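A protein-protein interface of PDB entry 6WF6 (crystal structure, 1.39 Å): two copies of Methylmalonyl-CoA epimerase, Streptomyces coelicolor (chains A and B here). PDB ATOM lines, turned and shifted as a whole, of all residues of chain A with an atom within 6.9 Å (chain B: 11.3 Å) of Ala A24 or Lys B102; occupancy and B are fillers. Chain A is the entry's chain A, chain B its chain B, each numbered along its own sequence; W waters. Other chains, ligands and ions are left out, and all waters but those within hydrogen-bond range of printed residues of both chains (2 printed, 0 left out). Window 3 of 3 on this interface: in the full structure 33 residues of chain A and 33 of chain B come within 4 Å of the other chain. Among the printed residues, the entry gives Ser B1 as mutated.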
ATOM      1  N   VAL A  19       0.199 -15.001  -0.066  1.00  0.00           N
ATOM      2  CA  VAL A  19       0.237 -14.814  -1.542  1.00  0.00           C
ATOM      3  C   VAL A  19       1.406 -15.615  -2.133  1.00  0.00           C
ATOM      4  O   VAL A  19       1.236 -16.322  -3.113  1.00  0.00           O
ATOM      5  CB  VAL A  19       0.356 -13.325  -1.888  1.00  0.00           C
ATOM      6  CG1 VAL A  19       0.824 -13.086  -3.312  1.00  0.00           C
ATOM      7  CG2 VAL A  19      -0.965 -12.614  -1.675  1.00  0.00           C
ATOM      8  N   GLU A  20       2.582 -15.516  -1.515  1.00  0.00           N
ATOM      9  CA  GLU A  20       3.763 -16.230  -2.042  1.00  0.00           C
ATOM     10  C   GLU A  20       3.573 -17.731  -1.940  1.00  0.00           C
ATOM     11  O   GLU A  20       3.963 -18.454  -2.880  1.00  0.00           O
ATOM     12  CB  GLU A  20       5.030 -15.761  -1.319  1.00  0.00           C
ATOM     13  CG  GLU A  20       6.278 -16.502  -1.723  1.00  0.00           C
ATOM     14  CD  GLU A  20       6.683 -16.428  -3.188  1.00  0.00           C
ATOM     15  OE1 GLU A  20       6.251 -15.516  -3.907  1.00  0.00           O
ATOM     16  OE2 GLU A  20       7.472 -17.292  -3.590  1.00  0.00           O
ATOM     17  N   PHE A  21       2.912 -18.216  -0.885  1.00  0.00           N
ATOM     18  CA  PHE A  21       2.602 -19.645  -0.798  1.00  0.00           C
ATOM     19  C   PHE A  21       1.733 -20.077  -1.993  1.00  0.00           C
ATOM     20  O   PHE A  21       1.995 -21.109  -2.667  1.00  0.00           O
ATOM     21  CB  PHE A  21       1.915 -19.964   0.527  1.00  0.00           C
ATOM     22  CG  PHE A  21       1.321 -21.342   0.537  1.00  0.00           C
ATOM     23  CD1 PHE A  21       2.122 -22.467   0.722  1.00  0.00           C
ATOM     24  CD2 PHE A  21      -0.035 -21.517   0.325  1.00  0.00           C
ATOM     25  CE1 PHE A  21       1.561 -23.734   0.644  1.00  0.00           C
ATOM     26  CE2 PHE A  21      -0.578 -22.793   0.237  1.00  0.00           C
ATOM     27  CZ  PHE A  21       0.230 -23.893   0.403  1.00  0.00           C
ATOM     28  N   TYR A  22       0.669 -19.330  -2.312  1.00  0.00           N
ATOM     29  CA  TYR A  22      -0.265 -19.733  -3.413  1.00  0.00           C
ATOM     30  C   TYR A  22       0.453 -19.644  -4.758  1.00  0.00           C
ATOM     31  O   TYR A  22       0.262 -20.494  -5.610  1.00  0.00           O
ATOM     32  CB  TYR A  22      -1.564 -18.916  -3.359  1.00  0.00           C
ATOM     33  CG  TYR A  22      -2.562 -19.477  -2.394  1.00  0.00           C
ATOM     34  CD1 TYR A  22      -3.439 -20.481  -2.774  1.00  0.00           C
ATOM     35  CD2 TYR A  22      -2.541 -19.130  -1.055  1.00  0.00           C
ATOM     36  CE1 TYR A  22      -4.324 -21.039  -1.876  1.00  0.00           C
ATOM     37  CE2 TYR A  22      -3.405 -19.708  -0.132  1.00  0.00           C
ATOM     38  CZ  TYR A  22      -4.284 -20.691  -0.528  1.00  0.00           C
ATOM     39  OH  TYR A  22      -5.138 -21.284   0.378  1.00  0.00           O
ATOM     40  N   ARG A  23       1.316 -18.647  -4.926  1.00  0.00           N
ATOM     41  CA  ARG A  23       2.121 -18.442  -6.169  1.00  0.00           C
ATOM     42  C   ARG A  23       3.120 -19.588  -6.351  1.00  0.00           C
ATOM     43  O   ARG A  23       3.155 -20.213  -7.424  1.00  0.00           O
ATOM     44  CB  ARG A  23       2.948 -17.152  -6.079  1.00  0.00           C
ATOM     45  CG  ARG A  23       3.108 -16.346  -7.366  1.00  0.00           C
ATOM     46  CD  ARG A  23       3.845 -17.011  -8.504  1.00  0.00           C
ATOM     47  NE  ARG A  23       5.235 -17.275  -8.178  1.00  0.00           N
ATOM     48  CZ  ARG A  23       6.023 -18.122  -8.807  1.00  0.00           C
ATOM     49  NH1 ARG A  23       7.227 -18.312  -8.323  1.00  0.00           N
ATOM     50  NH2 ARG A  23       5.615 -18.779  -9.883  1.00  0.00           N
ATOM     51  N   ALA A  24       3.899 -19.842  -5.327  1.00  0.00           N
ATOM     52  CA  ALA A  24       4.998 -20.829  -5.413  1.00  0.00           C
ATOM     53  C   ALA A  24       4.416 -22.228  -5.502  1.00  0.00           C
ATOM     54  O   ALA A  24       4.987 -23.079  -6.217  1.00  0.00           O
ATOM     55  CB  ALA A  24       5.943 -20.677  -4.264  1.00  0.00           C
ATOM     56  N   THR A  25       3.330 -22.542  -4.799  1.00  0.00           N
ATOM     57  CA  THR A  25       2.808 -23.922  -4.711  1.00  0.00           C
ATOM     58  C   THR A  25       1.949 -24.273  -5.923  1.00  0.00           C
ATOM     59  O   THR A  25       2.051 -25.386  -6.428  1.00  0.00           O
ATOM     60  CB  THR A  25       2.046 -24.151  -3.414  1.00  0.00           C
ATOM     61  OG1 THR A  25       2.856 -23.668  -2.328  1.00  0.00           O
ATOM     62  CG2 THR A  25       1.634 -25.608  -3.246  1.00  0.00           C
ATOM     63  N   TYR A  26       1.117 -23.350  -6.386  1.00  0.00           N
ATOM     64  CA  TYR A  26       0.073 -23.639  -7.390  1.00  0.00           C
ATOM     65  C   TYR A  26       0.247 -22.818  -8.655  1.00  0.00           C
ATOM     66  O   TYR A  26      -0.496 -23.102  -9.604  1.00  0.00           O
ATOM     67  CB  TYR A  26      -1.297 -23.321  -6.819  1.00  0.00           C
ATOM     68  CG  TYR A  26      -1.644 -23.934  -5.485  1.00  0.00           C
ATOM     69  CD1 TYR A  26      -1.572 -25.308  -5.282  1.00  0.00           C
ATOM     70  CD2 TYR A  26      -1.988 -23.152  -4.403  1.00  0.00           C
ATOM     71  CE1 TYR A  26      -1.870 -25.870  -4.061  1.00  0.00           C
ATOM     72  CE2 TYR A  26      -2.261 -23.702  -3.162  1.00  0.00           C
ATOM     73  CZ  TYR A  26      -2.260 -25.069  -3.007  1.00  0.00           C
ATOM     74  OH  TYR A  26      -2.597 -25.581  -1.781  1.00  0.00           O
ATOM     75  N   GLY A  27       1.120 -21.824  -8.660  1.00  0.00           N
ATOM     76  CA  GLY A  27       1.338 -20.983  -9.844  1.00  0.00           C
ATOM     77  C   GLY A  27       0.303 -19.895  -9.969  1.00  0.00           C
ATOM     78  O   GLY A  27       0.206 -19.279 -11.078  1.00  0.00           O
ATOM     79  N   PHE A  28      -0.476 -19.619  -8.929  1.00  0.00           N
ATOM     80  CA  PHE A  28      -1.507 -18.551  -8.971  1.00  0.00           C
ATOM     81  C   PHE A  28      -0.918 -17.146  -8.747  1.00  0.00           C
ATOM     82  O   PHE A  28      -0.393 -16.828  -7.660  1.00  0.00           O
ATOM     83  CB  PHE A  28      -2.567 -18.731  -7.897  1.00  0.00           C
ATOM     84  CG  PHE A  28      -3.340 -20.027  -7.921  1.00  0.00           C
ATOM     85  CD1 PHE A  28      -3.559 -20.722  -9.089  1.00  0.00           C
ATOM     86  CD2 PHE A  28      -3.877 -20.539  -6.756  1.00  0.00           C
ATOM     87  CE1 PHE A  28      -4.290 -21.897  -9.081  1.00  0.00           C
ATOM     88  CE2 PHE A  28      -4.594 -21.726  -6.743  1.00  0.00           C
ATOM     89  CZ  PHE A  28      -4.795 -22.415  -7.915  1.00  0.00           C
ATOM     90  N   SER B   1      -1.561 -28.639 -13.835  1.00  0.00           N
ATOM     91  CA  SER B   1      -1.841 -27.325 -13.247  1.00  0.00           C
ATOM     92  C   SER B   1      -3.301 -27.264 -12.788  1.00  0.00           C
ATOM     93  O   SER B   1      -4.188 -27.968 -13.288  1.00  0.00           O
ATOM     94  CB  SER B   1      -1.553 -26.203 -14.179  1.00  0.00           C
ATOM     95  OG  SER B   1      -2.519 -26.227 -15.210  1.00  0.00           O
ATOM     96  N   LEU B   2      -3.511 -26.402 -11.810  1.00  0.00           N
ATOM     97  CA  LEU B   2      -4.834 -26.192 -11.198  1.00  0.00           C
ATOM     98  C   LEU B   2      -5.592 -25.151 -12.035  1.00  0.00           C
ATOM     99  O   LEU B   2      -5.172 -23.996 -12.094  1.00  0.00           O
ATOM    100  CB  LEU B   2      -4.648 -25.781  -9.739  1.00  0.00           C
ATOM    101  CG  LEU B   2      -4.445 -26.918  -8.731  1.00  0.00           C
ATOM    102  CD1 LEU B   2      -3.228 -27.791  -9.007  1.00  0.00           C
ATOM    103  CD2 LEU B   2      -4.354 -26.316  -7.336  1.00  0.00           C
ATOM    104  N   ASP B  93      -2.581 -36.798 -10.159  1.00  0.00           N
ATOM    105  CA  ASP B  93      -1.338 -37.559  -9.776  1.00  0.00           C
ATOM    106  C   ASP B  93      -0.086 -36.706  -9.973  1.00  0.00           C
ATOM    107  O   ASP B  93       0.765 -36.668  -9.084  1.00  0.00           O
ATOM    108  CB  ASP B  93      -1.197 -38.879 -10.554  1.00  0.00           C
ATOM    109  CG  ASP B  93      -2.386 -39.812 -10.386  1.00  0.00           C
ATOM    110  OD1 ASP B  93      -3.418 -39.633 -11.082  1.00  0.00           O
ATOM    111  OD2 ASP B  93      -2.294 -40.687  -9.511  1.00  0.00           O
ATOM    112  N   ALA B  94       0.020 -36.074 -11.115  1.00  0.00           N
ATOM    113  CA  ALA B  94       1.203 -35.250 -11.464  1.00  0.00           C
ATOM    114  C   ALA B  94       1.244 -34.048 -10.530  1.00  0.00           C
ATOM    115  O   ALA B  94       2.286 -33.699  -9.993  1.00  0.00           O
ATOM    116  CB  ALA B  94       1.119 -34.790 -12.901  1.00  0.00           C
ATOM    117  N   ASP B  95       0.106 -33.396 -10.329  1.00  0.00           N
ATOM    118  CA  ASP B  95       0.107 -32.157  -9.519  1.00  0.00           C
ATOM    119  C   ASP B  95       0.369 -32.488  -8.056  1.00  0.00           C
ATOM    120  O   ASP B  95       1.141 -31.752  -7.414  1.00  0.00           O
ATOM    121  CB  ASP B  95      -1.189 -31.380  -9.731  1.00  0.00           C
ATOM    122  CG  ASP B  95      -1.159 -30.616 -11.036  1.00  0.00           C
ATOM    123  OD1 ASP B  95      -0.035 -30.274 -11.476  1.00  0.00           O
ATOM    124  OD2 ASP B  95      -2.207 -30.361 -11.623  1.00  0.00           O
ATOM    125  N   ALA B  96      -0.176 -33.579  -7.513  1.00  0.00           N
ATOM    126  CA  ALA B  96       0.126 -33.955  -6.124  1.00  0.00           C
ATOM    127  C   ALA B  96       1.621 -34.232  -5.974  1.00  0.00           C
ATOM    128  O   ALA B  96       2.212 -33.864  -4.968  1.00  0.00           O
ATOM    129  CB  ALA B  96      -0.653 -35.159  -5.678  1.00  0.00           C
ATOM    130  N   ALA B  97       2.221 -34.950  -6.935  1.00  0.00           N
ATOM    131  CA  ALA B  97       3.645 -35.295  -6.809  1.00  0.00           C
ATOM    132  C   ALA B  97       4.466 -34.005  -6.855  1.00  0.00           C
ATOM    133  O   ALA B  97       5.406 -33.865  -6.063  1.00  0.00           O
ATOM    134  CB  ALA B  97       4.061 -36.257  -7.889  1.00  0.00           C
ATOM    135  N   ASP B  98       4.128 -33.069  -7.735  1.00  0.00           N
ATOM    136  CA  ASP B  98       4.892 -31.796  -7.827  1.00  0.00           C
ATOM    137  C   ASP B  98       4.769 -31.026  -6.497  1.00  0.00           C
ATOM    138  O   ASP B  98       5.745 -30.433  -6.001  1.00  0.00           O
ATOM    139  CB  ASP B  98       4.435 -30.979  -9.022  1.00  0.00           C
ATOM    140  CG  ASP B  98       4.962 -31.499 -10.350  1.00  0.00           C
ATOM    141  OD1 ASP B  98       5.797 -32.445 -10.306  1.00  0.00           O
ATOM    142  OD2 ASP B  98       4.491 -31.005 -11.422  1.00  0.00           O
ATOM    143  N   ILE B  99       3.582 -30.993  -5.925  1.00  0.00           N
ATOM    144  CA  ILE B  99       3.332 -30.244  -4.675  1.00  0.00           C
ATOM    145  C   ILE B  99       4.015 -30.930  -3.484  1.00  0.00           C
ATOM    146  O   ILE B  99       4.640 -30.202  -2.666  1.00  0.00           O
ATOM    147  CB  ILE B  99       1.805 -30.063  -4.478  1.00  0.00           C
ATOM    148  CG1 ILE B  99       1.284 -29.080  -5.525  1.00  0.00           C
ATOM    149  CG2 ILE B  99       1.496 -29.598  -3.087  1.00  0.00           C
ATOM    150  CD1 ILE B  99      -0.221 -29.082  -5.712  1.00  0.00           C
ATOM    151  N   ARG B 100       4.029 -32.250  -3.433  1.00  0.00           N
ATOM    152  CA  ARG B 100       4.762 -32.932  -2.351  1.00  0.00           C
ATOM    153  C   ARG B 100       6.235 -32.530  -2.420  1.00  0.00           C
ATOM    154  O   ARG B 100       6.853 -32.286  -1.376  1.00  0.00           O
ATOM    155  CB  ARG B 100       4.612 -34.437  -2.478  1.00  0.00           C
ATOM    156  CG  ARG B 100       5.185 -35.165  -1.270  1.00  0.00           C
ATOM    157  CD  ARG B 100       5.119 -36.662  -1.425  1.00  0.00           C
ATOM    158  NE  ARG B 100       3.787 -37.233  -1.395  1.00  0.00           N
ATOM    159  CZ  ARG B 100       3.145 -37.702  -2.447  1.00  0.00           C
ATOM    160  NH1 ARG B 100       3.674 -37.628  -3.659  1.00  0.00           N
ATOM    161  NH2 ARG B 100       1.971 -38.286  -2.282  1.00  0.00           N
ATOM    162  N   ASP B 101       6.776 -32.480  -3.617  1.00  0.00           N
ATOM    163  CA  ASP B 101       8.222 -32.216  -3.846  1.00  0.00           C
ATOM    164  C   ASP B 101       8.553 -30.803  -3.381  1.00  0.00           C
ATOM    165  O   ASP B 101       9.748 -30.505  -3.140  1.00  0.00           O
ATOM    166  CB  ASP B 101       8.576 -32.386  -5.314  1.00  0.00           C
ATOM    167  CG  ASP B 101       8.710 -33.821  -5.773  1.00  0.00           C
ATOM    168  OD1 ASP B 101       8.711 -34.699  -4.900  1.00  0.00           O
ATOM    169  OD2 ASP B 101       8.735 -34.021  -7.021  1.00  0.00           O
ATOM    170  N   LYS B 102       7.573 -29.902  -3.308  1.00  0.00           N
ATOM    171  CA  LYS B 102       7.750 -28.533  -2.760  1.00  0.00           C
ATOM    172  C   LYS B 102       7.705 -28.481  -1.234  1.00  0.00           C
ATOM    173  O   LYS B 102       7.988 -27.432  -0.688  1.00  0.00           O
ATOM    174  CB  LYS B 102       6.725 -27.568  -3.368  1.00  0.00           C
ATOM    175  CG  LYS B 102       6.908 -27.335  -4.845  1.00  0.00           C
ATOM    176  CD  LYS B 102       5.894 -26.456  -5.501  1.00  0.00           C
ATOM    177  CE  LYS B 102       6.219 -26.317  -6.975  1.00  0.00           C
ATOM    178  NZ  LYS B 102       5.123 -25.639  -7.672  1.00  0.00           N
ATOM    179  N   GLY B 103       7.430 -29.581  -0.554  1.00  0.00           N
ATOM    180  CA  GLY B 103       7.413 -29.578   0.911  1.00  0.00           C
ATOM    181  C   GLY B 103       6.016 -29.462   1.474  1.00  0.00           C
ATOM    182  O   GLY B 103       5.907 -29.338   2.676  1.00  0.00           O
ATOM    183  N   VAL B 104       4.957 -29.595   0.665  1.00  0.00           N
ATOM    184  CA  VAL B 104       3.569 -29.651   1.170  1.00  0.00           C
ATOM    185  C   VAL B 104       3.119 -31.100   1.257  1.00  0.00           C
ATOM    186  O   VAL B 104       3.156 -31.780   0.211  1.00  0.00           O
ATOM    187  CB  VAL B 104       2.653 -28.837   0.242  1.00  0.00           C
ATOM    188  CG1 VAL B 104       1.202 -29.038   0.613  1.00  0.00           C
ATOM    189  CG2 VAL B 104       3.019 -27.373   0.325  1.00  0.00           C
ATOM    190  N   ARG B 105       2.774 -31.601   2.441  1.00  0.00           N
ATOM    191  CA  ARG B 105       2.423 -33.005   2.609  1.00  0.00           C
ATOM    192  C   ARG B 105       1.114 -33.325   1.907  1.00  0.00           C
ATOM    193  O   ARG B 105       0.141 -32.537   1.990  1.00  0.00           O
ATOM    194  CB  ARG B 105       2.361 -33.349   4.089  1.00  0.00           C
ATOM    195  CG  ARG B 105       3.744 -33.317   4.719  1.00  0.00           C
ATOM    196  CD  ARG B 105       3.587 -33.459   6.196  1.00  0.00           C
ATOM    197  NE  ARG B 105       3.046 -32.223   6.754  1.00  0.00           N
ATOM    198  CZ  ARG B 105       2.501 -32.107   7.934  1.00  0.00           C
ATOM    199  NH1 ARG B 105       2.344 -33.177   8.710  1.00  0.00           N
ATOM    200  NH2 ARG B 105       2.128 -30.920   8.348  1.00  0.00           N
ATOM    201  N   VAL B 106       1.037 -34.502   1.315  1.00  0.00           N
ATOM    202  CA  VAL B 106      -0.150 -35.082   0.671  1.00  0.00           C
ATOM    203  C   VAL B 106      -0.704 -36.193   1.575  1.00  0.00           C
ATOM    204  O   VAL B 106       0.009 -37.071   2.032  1.00  0.00           O
ATOM    205  CB  VAL B 106       0.220 -35.559  -0.741  1.00  0.00           C
ATOM    206  CG1 VAL B 106      -0.910 -36.277  -1.418  1.00  0.00           C
ATOM    207  CG2 VAL B 106       0.765 -34.400  -1.560  1.00  0.00           C
ATOM    208  N   LEU B 123      -4.246 -32.122   0.447  1.00  0.00           N
ATOM    209  CA  LEU B 123      -3.007 -31.518   0.952  1.00  0.00           C
ATOM    210  C   LEU B 123      -3.182 -31.215   2.446  1.00  0.00           C
ATOM    211  O   LEU B 123      -4.296 -30.820   2.880  1.00  0.00           O
ATOM    212  CB  LEU B 123      -2.687 -30.272   0.147  1.00  0.00           C
ATOM    213  CG  LEU B 123      -2.675 -30.408  -1.358  1.00  0.00           C
ATOM    214  CD1 LEU B 123      -2.363 -29.063  -1.994  1.00  0.00           C
ATOM    215  CD2 LEU B 123      -1.666 -31.508  -1.762  1.00  0.00           C
ATOM    216  N   HIS B 124      -2.120 -31.313   3.228  1.00  0.00           N
ATOM    217  CA  HIS B 124      -2.218 -31.114   4.680  1.00  0.00           C
ATOM    218  C   HIS B 124      -2.564 -29.664   5.028  1.00  0.00           C
ATOM    219  O   HIS B 124      -1.844 -28.717   4.680  1.00  0.00           O
ATOM    220  CB  HIS B 124      -0.874 -31.489   5.315  1.00  0.00           C
ATOM    221  CG  HIS B 124      -1.001 -31.818   6.765  1.00  0.00           C
ATOM    222  ND1 HIS B 124      -1.449 -30.915   7.703  1.00  0.00           N
ATOM    223  CD2 HIS B 124      -0.789 -32.983   7.425  1.00  0.00           C
ATOM    224  CE1 HIS B 124      -1.521 -31.489   8.893  1.00  0.00           C
ATOM    225  NE2 HIS B 124      -1.109 -32.793   8.744  1.00  0.00           N
ATOM    226  N   ASP B 127       0.113 -27.259   6.311  1.00  0.00           N
ATOM    227  CA  ASP B 127       1.086 -26.831   5.281  1.00  0.00           C
ATOM    228  C   ASP B 127       0.432 -25.842   4.313  1.00  0.00           C
ATOM    229  O   ASP B 127       1.150 -25.301   3.468  1.00  0.00           O
ATOM    230  CB  ASP B 127       1.646 -28.053   4.564  1.00  0.00           C
ATOM    231  CG  ASP B 127       2.463 -29.001   5.451  1.00  0.00           C
ATOM    232  OD1 ASP B 127       2.770 -28.646   6.598  1.00  0.00           O
ATOM    233  OD2 ASP B 127       2.747 -30.096   4.981  1.00  0.00           O
ATOM    234  N   CYS B 128      -0.877 -25.568   4.443  1.00  0.00           N
ATOM    235  CA  CYS B 128      -1.618 -24.695   3.504  1.00  0.00           C
ATOM    236  C   CYS B 128      -2.230 -23.502   4.244  1.00  0.00           C
ATOM    237  O   CYS B 128      -3.355 -23.095   3.906  1.00  0.00           O
ATOM    238  CB  CYS B 128      -2.676 -25.496   2.775  1.00  0.00           C
ATOM    239  SG  CYS B 128      -2.057 -26.822   1.719  1.00  0.00           S
ATOM    240  N   HIS B 129      -1.578 -22.980   5.274  1.00  0.00           N
ATOM    241  CA  HIS B 129      -2.077 -21.801   6.014  1.00  0.00           C
ATOM    242  C   HIS B 129      -3.519 -22.075   6.489  1.00  0.00           C
ATOM    243  O   HIS B 129      -4.363 -21.152   6.473  1.00  0.00           O
ATOM    244  CB  HIS B 129      -1.924 -20.520   5.196  1.00  0.00           C
ATOM    245  CG  HIS B 129      -0.513 -20.096   5.043  1.00  0.00           C
ATOM    246  ND1 HIS B 129       0.089 -19.359   6.035  1.00  0.00           N
ATOM    247  CD2 HIS B 129       0.427 -20.382   4.124  1.00  0.00           C
ATOM    248  CE1 HIS B 129       1.344 -19.126   5.666  1.00  0.00           C
ATOM    249  NE2 HIS B 129       1.585 -19.742   4.494  1.00  0.00           N
ATOM    250  N   LEU B 135      -7.451 -31.777  -4.362  1.00  0.00           N
ATOM    251  CA  LEU B 135      -7.186 -31.727  -5.798  1.00  0.00           C
ATOM    252  C   LEU B 135      -8.080 -32.757  -6.461  1.00  0.00           C
ATOM    253  O   LEU B 135      -8.133 -33.899  -5.925  1.00  0.00           O
ATOM    254  CB  LEU B 135      -5.714 -32.035  -6.075  1.00  0.00           C
ATOM    255  CG  LEU B 135      -4.696 -31.209  -5.293  1.00  0.00           C
ATOM    256  CD1 LEU B 135      -3.269 -31.624  -5.713  1.00  0.00           C
ATOM    257  CD2 LEU B 135      -4.867 -29.712  -5.549  1.00  0.00           C
HETATM  258  O   HOH W   1      -1.009 -25.481 -10.589  1.00  0.00           O
HETATM  259  O   HOH W   2      -4.460 -20.659   2.903  1.00  0.00           O
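NZ of Lys B102 is in hydrogen-bond range of O of Thr A25 (3.3 Å).
The side-chain sulfur (SG) of Cys B128 is in hydrogen-bond range of the side-chain hydroxyl (OH) of Tyr A26 (3.8 Å).
The backbone carbonyl oxygen (O) of Ala A24 sits at hydrogen-bond distance from the side-chain amino group (NZ) of Lys B102 (2.9 Å).
O of Phe A21 lies within hydrogen-bond range of OG1 of Thr A25 (2.7 Å).
The backbone NH (N) of Val B104 lies within hydrogen-bond range of the backbone carbonyl oxygen (O) of Ile B99, 3.4 Å away.
The guanidinium group (NE) of Arg B105 is in salt-bridge range of the side-chain carboxylate (OD2) of Asp B127 (2.8 Å).
O of His B124 is in hydrogen-bond range of SG of Cys B128, at 3.5 Å.
Among the printed residues, merely in contact across the chains: Phe A21 with Val B104, Phe A21 with Asp B127, Phe A21 with Cys B128, Phe A21 with His B129, Thr A25 with Ile B99, Tyr A26 with Leu B2, Tyr A26 with Ile B99, Tyr A26 with Leu B123 and Phe A28 with Leu B2.
No residue of chain B comes within 4 Å of Glu A20.
Of the printed residues of chain B, Phe A21 touches Val B104 (3.9 Å), Asp B127 (3.3 Å), Cys B128 (3.7 Å) and His B129 (3.8 Å).
Ala A24 touches just one residue of chain B: Lys B102.
No residue of chain B comes within 4 Å of Gly A27.
Of the printed residues of chain B, Phe A28 touches Leu B2 (3.8 Å).
Printed residues of chain A within 4 Å of Leu B2: Tyr A26 and Phe A28.
Printed residues of chain A within 4 Å of Ile B99: Thr A25 and Tyr A26.
Of the printed residues of chain A, Lys B102 touches Ala A24 (2.9 Å) and Thr A25 (3.3 Å).
Of the printed residues of chain A, His B129 touches Phe A21.
The nearest residue of chain B that does not touch Ala A24 is Ile B99 (7.1 Å).
The nearest residue of chain A that does not touch Lys B102 is Tyr A26 (4.8 Å).
Printed residues of chain A that touch a printed residue of chain B: Phe A21, Ala A24, Thr A25, Tyr A26 and Phe A28.
Along chain A the printed residues that touch a printed residue of chain B span positions 21 to 28.
Among the printed residues, no Asp or Glu carboxylate lies within 4 Å of a Lys or Arg side-chain nitrogen of the other chain.
No position is printed for both chains.
Of the 12 pairs that touch across the chains among the printed residues, none has its exchanged pair printed and touching as well.
Water W1 bridges O of Tyr A26 (2.6 Å) and N of Leu B2 (2.9 Å).
Water W2 lies within hydrogen-bond range of OH of Tyr A22 (2.7 Å) and O of Cys B128 (2.9 Å).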
